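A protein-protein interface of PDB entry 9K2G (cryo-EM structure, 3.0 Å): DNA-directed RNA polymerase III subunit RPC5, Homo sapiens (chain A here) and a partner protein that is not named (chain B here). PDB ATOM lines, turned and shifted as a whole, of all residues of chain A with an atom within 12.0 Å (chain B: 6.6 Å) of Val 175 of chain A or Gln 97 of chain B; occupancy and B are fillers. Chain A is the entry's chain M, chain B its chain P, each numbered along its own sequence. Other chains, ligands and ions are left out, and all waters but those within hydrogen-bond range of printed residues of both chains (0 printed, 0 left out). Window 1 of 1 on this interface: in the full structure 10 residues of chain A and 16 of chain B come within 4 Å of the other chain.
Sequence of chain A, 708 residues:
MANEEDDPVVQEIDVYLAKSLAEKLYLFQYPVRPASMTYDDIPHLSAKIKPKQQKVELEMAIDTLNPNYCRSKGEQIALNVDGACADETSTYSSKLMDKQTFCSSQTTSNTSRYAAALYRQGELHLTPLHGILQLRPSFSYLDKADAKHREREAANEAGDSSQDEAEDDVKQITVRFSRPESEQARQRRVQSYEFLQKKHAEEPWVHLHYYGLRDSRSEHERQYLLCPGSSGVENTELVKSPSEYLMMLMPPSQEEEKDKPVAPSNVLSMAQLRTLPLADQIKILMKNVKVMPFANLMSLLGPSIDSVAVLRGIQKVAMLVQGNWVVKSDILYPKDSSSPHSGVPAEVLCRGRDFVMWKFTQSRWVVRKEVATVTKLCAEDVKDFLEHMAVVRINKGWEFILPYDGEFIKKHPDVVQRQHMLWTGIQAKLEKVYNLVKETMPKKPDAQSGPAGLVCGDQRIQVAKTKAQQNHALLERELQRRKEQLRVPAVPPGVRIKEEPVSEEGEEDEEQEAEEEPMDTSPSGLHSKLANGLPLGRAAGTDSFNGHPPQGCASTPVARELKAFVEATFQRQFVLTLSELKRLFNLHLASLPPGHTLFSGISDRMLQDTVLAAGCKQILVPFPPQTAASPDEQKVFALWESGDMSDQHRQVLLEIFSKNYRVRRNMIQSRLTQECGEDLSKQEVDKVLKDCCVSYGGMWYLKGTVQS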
ATOM      1  N   VAL A 170     -24.607  -7.163 -25.220  1.00  0.00           N
ATOM      2  CA  VAL A 170     -25.065  -6.017 -24.451  1.00  0.00           C
ATOM      3  C   VAL A 170     -24.714  -6.236 -22.994  1.00  0.00           C
ATOM      4  O   VAL A 170     -25.000  -7.296 -22.416  1.00  0.00           O
ATOM      5  CB  VAL A 170     -26.572  -5.799 -24.654  1.00  0.00           C
ATOM      6  CG1 VAL A 170     -26.843  -5.291 -26.064  1.00  0.00           C
ATOM      7  CG2 VAL A 170     -27.347  -7.087 -24.398  1.00  0.00           C
ATOM      8  N   LYS A 171     -24.067  -5.245 -22.389  1.00  0.00           N
ATOM      9  CA  LYS A 171     -23.637  -5.403 -21.006  1.00  0.00           C
ATOM     10  C   LYS A 171     -24.865  -5.381 -20.108  1.00  0.00           C
ATOM     11  O   LYS A 171     -25.352  -4.310 -19.733  1.00  0.00           O
ATOM     12  CB  LYS A 171     -22.646  -4.309 -20.606  1.00  0.00           C
ATOM     13  CG  LYS A 171     -21.313  -4.391 -21.326  1.00  0.00           C
ATOM     14  CD  LYS A 171     -20.167  -3.927 -20.437  1.00  0.00           C
ATOM     15  CE  LYS A 171     -20.435  -2.551 -19.850  1.00  0.00           C
ATOM     16  NZ  LYS A 171     -20.606  -1.520 -20.906  1.00  0.00           N
ATOM     17  N   GLN A 172     -25.388  -6.571 -19.800  1.00  0.00           N
ATOM     18  CA  GLN A 172     -26.508  -6.684 -18.881  1.00  0.00           C
ATOM     19  C   GLN A 172     -26.188  -5.925 -17.604  1.00  0.00           C
ATOM     20  O   GLN A 172     -25.045  -5.912 -17.141  1.00  0.00           O
ATOM     21  CB  GLN A 172     -26.797  -8.150 -18.573  1.00  0.00           C
ATOM     22  CG  GLN A 172     -28.043  -8.389 -17.736  1.00  0.00           C
ATOM     23  CD  GLN A 172     -28.139  -9.816 -17.223  1.00  0.00           C
ATOM     24  OE1 GLN A 172     -27.276 -10.649 -17.497  1.00  0.00           O
ATOM     25  NE2 GLN A 172     -29.195 -10.101 -16.466  1.00  0.00           N
ATOM     26  N   ILE A 173     -27.211  -5.299 -17.023  1.00  0.00           N
ATOM     27  CA  ILE A 173     -26.950  -4.354 -15.946  1.00  0.00           C
ATOM     28  C   ILE A 173     -26.534  -5.140 -14.707  1.00  0.00           C
ATOM     29  O   ILE A 173     -27.369  -5.554 -13.897  1.00  0.00           O
ATOM     30  CB  ILE A 173     -28.186  -3.484 -15.664  1.00  0.00           C
ATOM     31  CG1 ILE A 173     -28.653  -2.812 -16.960  1.00  0.00           C
ATOM     32  CG2 ILE A 173     -27.879  -2.418 -14.636  1.00  0.00           C
ATOM     33  CD1 ILE A 173     -29.915  -1.998 -16.821  1.00  0.00           C
ATOM     34  N   THR A 174     -25.227  -5.337 -14.564  1.00  0.00           N
ATOM     35  CA  THR A 174     -24.647  -5.981 -13.389  1.00  0.00           C
ATOM     36  C   THR A 174     -24.221  -4.946 -12.362  1.00  0.00           C
ATOM     37  O   THR A 174     -23.092  -4.951 -11.871  1.00  0.00           O
ATOM     38  CB  THR A 174     -23.471  -6.861 -13.797  1.00  0.00           C
ATOM     39  OG1 THR A 174     -22.523  -6.087 -14.544  1.00  0.00           O
ATOM     40  CG2 THR A 174     -23.966  -7.998 -14.663  1.00  0.00           C
ATOM     41  N   VAL A 175     -25.128  -4.036 -12.015  1.00  0.00           N
ATOM     42  CA  VAL A 175     -24.856  -3.119 -10.919  1.00  0.00           C
ATOM     43  C   VAL A 175     -24.881  -3.922  -9.625  1.00  0.00           C
ATOM     44  O   VAL A 175     -25.901  -4.518  -9.263  1.00  0.00           O
ATOM     45  CB  VAL A 175     -25.863  -1.964 -10.902  1.00  0.00           C
ATOM     46  CG1 VAL A 175     -25.495  -0.944 -11.969  1.00  0.00           C
ATOM     47  CG2 VAL A 175     -27.279  -2.478 -11.131  1.00  0.00           C
ATOM     48  N   ARG A 176     -23.747  -3.969  -8.940  1.00  0.00           N
ATOM     49  CA  ARG A 176     -23.588  -4.870  -7.807  1.00  0.00           C
ATOM     50  C   ARG A 176     -24.041  -4.217  -6.510  1.00  0.00           C
ATOM     51  O   ARG A 176     -23.917  -3.000  -6.333  1.00  0.00           O
ATOM     52  CB  ARG A 176     -22.134  -5.321  -7.675  1.00  0.00           C
ATOM     53  CG  ARG A 176     -21.764  -6.475  -8.581  1.00  0.00           C
ATOM     54  CD  ARG A 176     -20.398  -7.024  -8.219  1.00  0.00           C
ATOM     55  NE  ARG A 176     -20.167  -8.335  -8.822  1.00  0.00           N
ATOM     56  CZ  ARG A 176     -19.087  -9.073  -8.610  1.00  0.00           C
ATOM     57  NH1 ARG A 176     -18.112  -8.664  -7.815  1.00  0.00           N
ATOM     58  NH2 ARG A 176     -18.984 -10.257  -9.209  1.00  0.00           N
ATOM     59  N   PHE A 177     -24.587  -5.037  -5.612  1.00  0.00           N
ATOM     60  CA  PHE A 177     -24.895  -4.570  -4.271  1.00  0.00           C
ATOM     61  C   PHE A 177     -23.633  -4.059  -3.600  1.00  0.00           C
ATOM     62  O   PHE A 177     -22.621  -4.761  -3.543  1.00  0.00           O
ATOM     63  CB  PHE A 177     -25.497  -5.705  -3.440  1.00  0.00           C
ATOM     64  CG  PHE A 177     -26.973  -5.879  -3.628  1.00  0.00           C
ATOM     65  CD1 PHE A 177     -27.675  -5.098  -4.529  1.00  0.00           C
ATOM     66  CD2 PHE A 177     -27.664  -6.816  -2.887  1.00  0.00           C
ATOM     67  CE1 PHE A 177     -29.032  -5.266  -4.691  1.00  0.00           C
ATOM     68  CE2 PHE A 177     -29.019  -6.986  -3.040  1.00  0.00           C
ATOM     69  CZ  PHE A 177     -29.704  -6.210  -3.941  1.00  0.00           C
ATOM     70  N   SER A 178     -23.690  -2.826  -3.096  1.00  0.00           N
ATOM     71  CA  SER A 178     -22.605  -2.296  -2.281  1.00  0.00           C
ATOM     72  C   SER A 178     -22.729  -2.974  -0.918  1.00  0.00           C
ATOM     73  O   SER A 178     -23.263  -2.416   0.042  1.00  0.00           O
ATOM     74  CB  SER A 178     -22.668  -0.777  -2.182  1.00  0.00           C
ATOM     75  OG  SER A 178     -23.866  -0.357  -1.551  1.00  0.00           O
ATOM     76  N   ARG A 179     -22.256  -4.209  -0.866  1.00  0.00           N
ATOM     77  CA  ARG A 179     -22.400  -5.018   0.330  1.00  0.00           C
ATOM     78  C   ARG A 179     -21.744  -4.312   1.510  1.00  0.00           C
ATOM     79  O   ARG A 179     -20.572  -3.915   1.411  1.00  0.00           O
ATOM     80  CB  ARG A 179     -21.767  -6.397   0.131  1.00  0.00           C
ATOM     81  CG  ARG A 179     -22.522  -7.350  -0.777  1.00  0.00           C
ATOM     82  CD  ARG A 179     -21.872  -8.732  -0.732  1.00  0.00           C
ATOM     83  NE  ARG A 179     -22.607  -9.734  -1.497  1.00  0.00           N
ATOM     84  CZ  ARG A 179     -22.336 -11.034  -1.481  1.00  0.00           C
ATOM     85  NH1 ARG A 179     -21.370 -11.530  -0.729  1.00  0.00           N
ATOM     86  NH2 ARG A 179     -23.050 -11.855  -2.247  1.00  0.00           N
ATOM     87  N   PRO A 180     -22.448  -4.125   2.626  1.00  0.00           N
ATOM     88  CA  PRO A 180     -21.793  -3.549   3.803  1.00  0.00           C
ATOM     89  C   PRO A 180     -20.683  -4.462   4.292  1.00  0.00           C
ATOM     90  O   PRO A 180     -20.935  -5.550   4.821  1.00  0.00           O
ATOM     91  CB  PRO A 180     -22.932  -3.425   4.823  1.00  0.00           C
ATOM     92  CG  PRO A 180     -23.978  -4.367   4.350  1.00  0.00           C
ATOM     93  CD  PRO A 180     -23.873  -4.403   2.858  1.00  0.00           C
ATOM     94  N   LEU B  63     -25.961   7.554 -12.097  1.00  0.00           N
ATOM     95  CA  LEU B  63     -26.125   7.092 -13.467  1.00  0.00           C
ATOM     96  C   LEU B  63     -25.665   5.649 -13.599  1.00  0.00           C
ATOM     97  O   LEU B  63     -24.817   5.169 -12.842  1.00  0.00           O
ATOM     98  CB  LEU B  63     -25.348   7.971 -14.457  1.00  0.00           C
ATOM     99  CG  LEU B  63     -25.898   9.367 -14.747  1.00  0.00           C
ATOM    100  CD1 LEU B  63     -25.119  10.016 -15.878  1.00  0.00           C
ATOM    101  CD2 LEU B  63     -27.384   9.313 -15.077  1.00  0.00           C
ATOM    102  N   ASP B  64     -26.248   4.961 -14.579  1.00  0.00           N
ATOM    103  CA  ASP B  64     -25.863   3.612 -14.958  1.00  0.00           C
ATOM    104  C   ASP B  64     -25.586   3.581 -16.453  1.00  0.00           C
ATOM    105  O   ASP B  64     -26.209   4.305 -17.239  1.00  0.00           O
ATOM    106  CB  ASP B  64     -26.950   2.585 -14.600  1.00  0.00           C
ATOM    107  CG  ASP B  64     -27.010   2.296 -13.112  1.00  0.00           C
ATOM    108  OD1 ASP B  64     -25.964   2.421 -12.438  1.00  0.00           O
ATOM    109  OD2 ASP B  64     -28.100   1.938 -12.615  1.00  0.00           O
ATOM    110  N   LEU B  65     -24.643   2.722 -16.840  1.00  0.00           N
ATOM    111  CA  LEU B  65     -24.153   2.640 -18.207  1.00  0.00           C
ATOM    112  C   LEU B  65     -24.752   1.429 -18.907  1.00  0.00           C
ATOM    113  O   LEU B  65     -24.752   0.322 -18.355  1.00  0.00           O
ATOM    114  CB  LEU B  65     -22.624   2.553 -18.223  1.00  0.00           C
ATOM    115  CG  LEU B  65     -21.966   2.497 -19.607  1.00  0.00           C
ATOM    116  CD1 LEU B  65     -21.973   3.866 -20.277  1.00  0.00           C
ATOM    117  CD2 LEU B  65     -20.550   1.946 -19.504  1.00  0.00           C
ATOM    118  N   ARG B  75     -28.276   6.195 -18.162  1.00  0.00           N
ATOM    119  CA  ARG B  75     -29.620   6.204 -17.611  1.00  0.00           C
ATOM    120  C   ARG B  75     -29.581   6.597 -16.144  1.00  0.00           C
ATOM    121  O   ARG B  75     -28.636   6.269 -15.423  1.00  0.00           O
ATOM    122  CB  ARG B  75     -30.287   4.827 -17.763  1.00  0.00           C
ATOM    123  CG  ARG B  75     -31.761   4.795 -17.393  1.00  0.00           C
ATOM    124  CD  ARG B  75     -32.286   3.368 -17.386  1.00  0.00           C
ATOM    125  NE  ARG B  75     -31.626   2.560 -16.368  1.00  0.00           N
ATOM    126  CZ  ARG B  75     -31.800   1.256 -16.223  1.00  0.00           C
ATOM    127  NH1 ARG B  75     -32.594   0.566 -17.027  1.00  0.00           N
ATOM    128  NH2 ARG B  75     -31.157   0.620 -15.245  1.00  0.00           N
ATOM    129  N   LYS B  77     -30.364   6.369 -12.279  1.00  0.00           N
ATOM    130  CA  LYS B  77     -30.567   5.223 -11.407  1.00  0.00           C
ATOM    131  C   LYS B  77     -31.970   5.262 -10.810  1.00  0.00           C
ATOM    132  O   LYS B  77     -32.468   6.324 -10.428  1.00  0.00           O
ATOM    133  CB  LYS B  77     -29.513   5.193 -10.303  1.00  0.00           C
ATOM    134  CG  LYS B  77     -29.407   3.858  -9.577  1.00  0.00           C
ATOM    135  CD  LYS B  77     -28.096   3.737  -8.822  1.00  0.00           C
ATOM    136  CE  LYS B  77     -27.949   2.367  -8.185  1.00  0.00           C
ATOM    137  NZ  LYS B  77     -26.610   2.193  -7.551  1.00  0.00           N
ATOM    138  N   GLU B  92     -33.137   0.530   0.033  1.00  0.00           N
ATOM    139  CA  GLU B  92     -34.297   0.127  -0.756  1.00  0.00           C
ATOM    140  C   GLU B  92     -33.885  -0.238  -2.177  1.00  0.00           C
ATOM    141  O   GLU B  92     -34.205  -1.321  -2.674  1.00  0.00           O
ATOM    142  CB  GLU B  92     -35.331   1.248  -0.763  1.00  0.00           C
ATOM    143  CG  GLU B  92     -36.584   0.943  -1.549  1.00  0.00           C
ATOM    144  CD  GLU B  92     -37.399   2.186  -1.818  1.00  0.00           C
ATOM    145  OE1 GLU B  92     -36.805   3.220  -2.179  1.00  0.00           O
ATOM    146  OE2 GLU B  92     -38.634   2.135  -1.653  1.00  0.00           O
ATOM    147  N   LYS B  93     -33.148   0.658  -2.840  1.00  0.00           N
ATOM    148  CA  LYS B  93     -32.660   0.335  -4.176  1.00  0.00           C
ATOM    149  C   LYS B  93     -31.573  -0.738  -4.134  1.00  0.00           C
ATOM    150  O   LYS B  93     -31.459  -1.527  -5.071  1.00  0.00           O
ATOM    151  CB  LYS B  93     -32.167   1.598  -4.892  1.00  0.00           C
ATOM    152  CG  LYS B  93     -31.026   2.338  -4.212  1.00  0.00           C
ATOM    153  CD  LYS B  93     -29.670   1.924  -4.767  1.00  0.00           C
ATOM    154  CE  LYS B  93     -28.544   2.673  -4.078  1.00  0.00           C
ATOM    155  NZ  LYS B  93     -27.210   2.224  -4.570  1.00  0.00           N
ATOM    156  N   LEU B  94     -30.798  -0.804  -3.046  1.00  0.00           N
ATOM    157  CA  LEU B  94     -29.763  -1.813  -2.861  1.00  0.00           C
ATOM    158  C   LEU B  94     -30.328  -3.169  -2.463  1.00  0.00           C
ATOM    159  O   LEU B  94     -29.564  -4.051  -2.064  1.00  0.00           O
ATOM    160  CB  LEU B  94     -28.766  -1.342  -1.801  1.00  0.00           C
ATOM    161  CG  LEU B  94     -27.348  -1.915  -1.858  1.00  0.00           C
ATOM    162  CD1 LEU B  94     -26.596  -1.358  -3.052  1.00  0.00           C
ATOM    163  CD2 LEU B  94     -26.615  -1.633  -0.556  1.00  0.00           C
ATOM    164  N   VAL B  95     -31.648  -3.301  -2.448  1.00  0.00           N
ATOM    165  CA  VAL B  95     -32.320  -4.598  -2.456  1.00  0.00           C
ATOM    166  C   VAL B  95     -33.061  -4.821  -3.773  1.00  0.00           C
ATOM    167  O   VAL B  95     -32.931  -5.879  -4.407  1.00  0.00           O
ATOM    168  CB  VAL B  95     -33.277  -4.729  -1.251  1.00  0.00           C
ATOM    169  CG1 VAL B  95     -34.063  -6.017  -1.350  1.00  0.00           C
ATOM    170  CG2 VAL B  95     -32.498  -4.669   0.059  1.00  0.00           C
ATOM    171  N   TYR B  96     -33.824  -3.818  -4.213  1.00  0.00           N
ATOM    172  CA  TYR B  96     -34.549  -3.920  -5.471  1.00  0.00           C
ATOM    173  C   TYR B  96     -33.627  -4.176  -6.656  1.00  0.00           C
ATOM    174  O   TYR B  96     -34.071  -4.735  -7.662  1.00  0.00           O
ATOM    175  CB  TYR B  96     -35.356  -2.644  -5.695  1.00  0.00           C
ATOM    176  CG  TYR B  96     -36.260  -2.654  -6.906  1.00  0.00           C
ATOM    177  CD1 TYR B  96     -35.813  -2.188  -8.139  1.00  0.00           C
ATOM    178  CD2 TYR B  96     -37.568  -3.102  -6.806  1.00  0.00           C
ATOM    179  CE1 TYR B  96     -36.643  -2.187  -9.244  1.00  0.00           C
ATOM    180  CE2 TYR B  96     -38.404  -3.099  -7.896  1.00  0.00           C
ATOM    181  CZ  TYR B  96     -37.945  -2.646  -9.111  1.00  0.00           C
ATOM    182  OH  TYR B  96     -38.795  -2.655 -10.189  1.00  0.00           O
ATOM    183  N   GLN B  97     -32.349  -3.807  -6.549  1.00  0.00           N
ATOM    184  CA  GLN B  97     -31.420  -3.955  -7.664  1.00  0.00           C
ATOM    185  C   GLN B  97     -31.194  -5.421  -8.017  1.00  0.00           C
ATOM    186  O   GLN B  97     -31.385  -5.833  -9.169  1.00  0.00           O
ATOM    187  CB  GLN B  97     -30.111  -3.254  -7.296  1.00  0.00           C
ATOM    188  CG  GLN B  97     -28.916  -3.534  -8.171  1.00  0.00           C
ATOM    189  CD  GLN B  97     -27.688  -2.810  -7.652  1.00  0.00           C
ATOM    190  OE1 GLN B  97     -26.872  -3.386  -6.930  1.00  0.00           O
ATOM    191  NE2 GLN B  97     -27.559  -1.536  -8.001  1.00  0.00           N
ATOM    192  N   ILE B  98     -30.817  -6.244  -7.036  1.00  0.00           N
ATOM    193  CA  ILE B  98     -30.648  -7.664  -7.332  1.00  0.00           C
ATOM    194  C   ILE B  98     -31.988  -8.379  -7.380  1.00  0.00           C
ATOM    195  O   ILE B  98     -32.094  -9.428  -8.032  1.00  0.00           O
ATOM    196  CB  ILE B  98     -29.665  -8.327  -6.339  1.00  0.00           C
ATOM    197  CG1 ILE B  98     -28.222  -7.990  -6.731  1.00  0.00           C
ATOM    198  CG2 ILE B  98     -29.842  -9.842  -6.250  1.00  0.00           C
ATOM    199  CD1 ILE B  98     -27.179  -8.657  -5.867  1.00  0.00           C
ATOM    200  N   ILE B  99     -33.041  -7.819  -6.780  1.00  0.00           N
ATOM    201  CA  ILE B  99     -34.369  -8.368  -7.056  1.00  0.00           C
ATOM    202  C   ILE B  99     -34.661  -8.311  -8.555  1.00  0.00           C
ATOM    203  O   ILE B  99     -35.071  -9.303  -9.168  1.00  0.00           O
ATOM    204  CB  ILE B  99     -35.445  -7.634  -6.242  1.00  0.00           C
ATOM    205  CG1 ILE B  99     -35.302  -7.972  -4.756  1.00  0.00           C
ATOM    206  CG2 ILE B  99     -36.817  -8.013  -6.756  1.00  0.00           C
ATOM    207  CD1 ILE B  99     -36.270  -7.243  -3.858  1.00  0.00           C
ATOM    208  N   GLU B 100     -34.410  -7.151  -9.168  1.00  0.00           N
ATOM    209  CA  GLU B 100     -34.581  -7.010 -10.614  1.00  0.00           C
ATOM    210  C   GLU B 100     -33.596  -7.885 -11.377  1.00  0.00           C
ATOM    211  O   GLU B 100     -33.945  -8.461 -12.418  1.00  0.00           O
ATOM    212  CB  GLU B 100     -34.425  -5.541 -11.013  1.00  0.00           C
ATOM    213  CG  GLU B 100     -34.444  -5.288 -12.513  1.00  0.00           C
ATOM    214  CD  GLU B 100     -34.305  -3.819 -12.857  1.00  0.00           C
ATOM    215  OE1 GLU B 100     -34.087  -3.005 -11.935  1.00  0.00           O
ATOM    216  OE2 GLU B 100     -34.417  -3.475 -14.054  1.00  0.00           O
ATOM    217  N   ASP B 101     -32.357  -7.982 -10.889  1.00  0.00           N
ATOM    218  CA  ASP B 101     -31.359  -8.802 -11.572  1.00  0.00           C
ATOM    219  C   ASP B 101     -31.789 -10.261 -11.639  1.00  0.00           C
ATOM    220  O   ASP B 101     -31.640 -10.915 -12.680  1.00  0.00           O
ATOM    221  CB  ASP B 101     -30.004  -8.678 -10.867  1.00  0.00           C
ATOM    222  CG  ASP B 101     -29.414  -7.285 -10.968  1.00  0.00           C
ATOM    223  OD1 ASP B 101     -29.609  -6.633 -12.020  1.00  0.00           O
ATOM    224  OD2 ASP B 101     -28.763  -6.836 -10.005  1.00  0.00           O
ATOM    225  N   ALA B 102     -32.326 -10.791 -10.538  1.00  0.00           N
ATOM    226  CA  ALA B 102     -32.910 -12.130 -10.565  1.00  0.00           C
ATOM    227  C   ALA B 102     -34.106 -12.177 -11.505  1.00  0.00           C
ATOM    228  O   ALA B 102     -34.239 -13.108 -12.305  1.00  0.00           O
ATOM    229  CB  ALA B 102     -33.309 -12.555  -9.153  1.00  0.00           C
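The backbone carbonyl oxygen (O) of Val 175 of chain A sits close to the side-chain amide oxygen (OE1) of Gln 97 of chain B (2.8 Å).
The backbone carbonyl oxygen of Arg 176 of chain A lies close to the side-chain amide oxygen of Gln 97 of chain B.
The backbone NH of Phe 177 of chain A lies close to the side-chain amide oxygen of Gln 97 of chain B (3.1 Å).
OD1 of Asp 101 of chain B lies close to O of Ile 173 of chain A (3.1 Å).
The backbone carbonyl oxygen (O) of Arg 75 of chain B is in hydrogen-bond range of the backbone NH (N) of Asp 64 of chain B, 2.9 Å away.
Among the printed residues, merely in contact across the chains: Phe 177 of chain A with Leu 94 of chain B, Phe 177 of chain A with Ile 98 of chain B, Ser 178 of chain A with Leu 94 of chain B, Phe 177 of chain A with Val 95 of chain B, Ile 173 of chain A with Arg 75 of chain B, Val 175 of chain A with Asp 64 of chain B, Lys 171 of chain A with Leu 65 of chain B and Val 175 of chain A with Asp 101 of chain B.
Of the printed residues of chain A, Gln 97 of chain B touches Val 175, Arg 176 and Phe 177.
Of chain A, only Val 175 comes within 4 Å of Asp 64 of chain B.
No residue of chain A comes within 4 Å of Lys 93 of chain B.
Of chain A, only Phe 177 (2.9 Å) and Ser 178 (3.2 Å) come within 4 Å of Leu 94 of chain B.
Of the printed residues of chain A, Val 95 of chain B touches Phe 177 (3.3 Å).
Of the printed residues of chain A, Ile 98 of chain B touches Phe 177.
Glu 100 of chain B touches none of the printed residues of chain A.
Of the printed residues of chain B, Arg 176 of chain A touches Gln 97 (3.0 Å).
Printed residues of chain B within 4 Å of Ile 173 of chain A: Arg 75 (3.3 Å) and Asp 101 (3.1 Å).
Of the printed residues of chain B, Ser 178 of chain A touches Leu 94 (3.2 Å).
Thr 174 of chain A touches none of the printed residues of chain B.
Pro 180 of chain A touches none of the printed residues of chain B.
The nearest residue of chain A that does not touch Gln 97 of chain B is Ser 178 of chain A (5.0 Å).
The nearest printed residue of chain A that does not touch Leu 65 of chain B is Ile 173 of chain A (5.2 Å).
Hydrophobic or aromatic side chains of chain A that line the printed part of chain B: Ile 173, Val 175 and Phe 177.
Of the 16 printed residues of chain B, 8 touch a printed residue of chain A.
Hydrophobic or aromatic side chains of chain B that line the printed part of chain A: Leu 65, Leu 94 and Ile 98.
Among the printed residues, 12 pairs touch across the chains.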
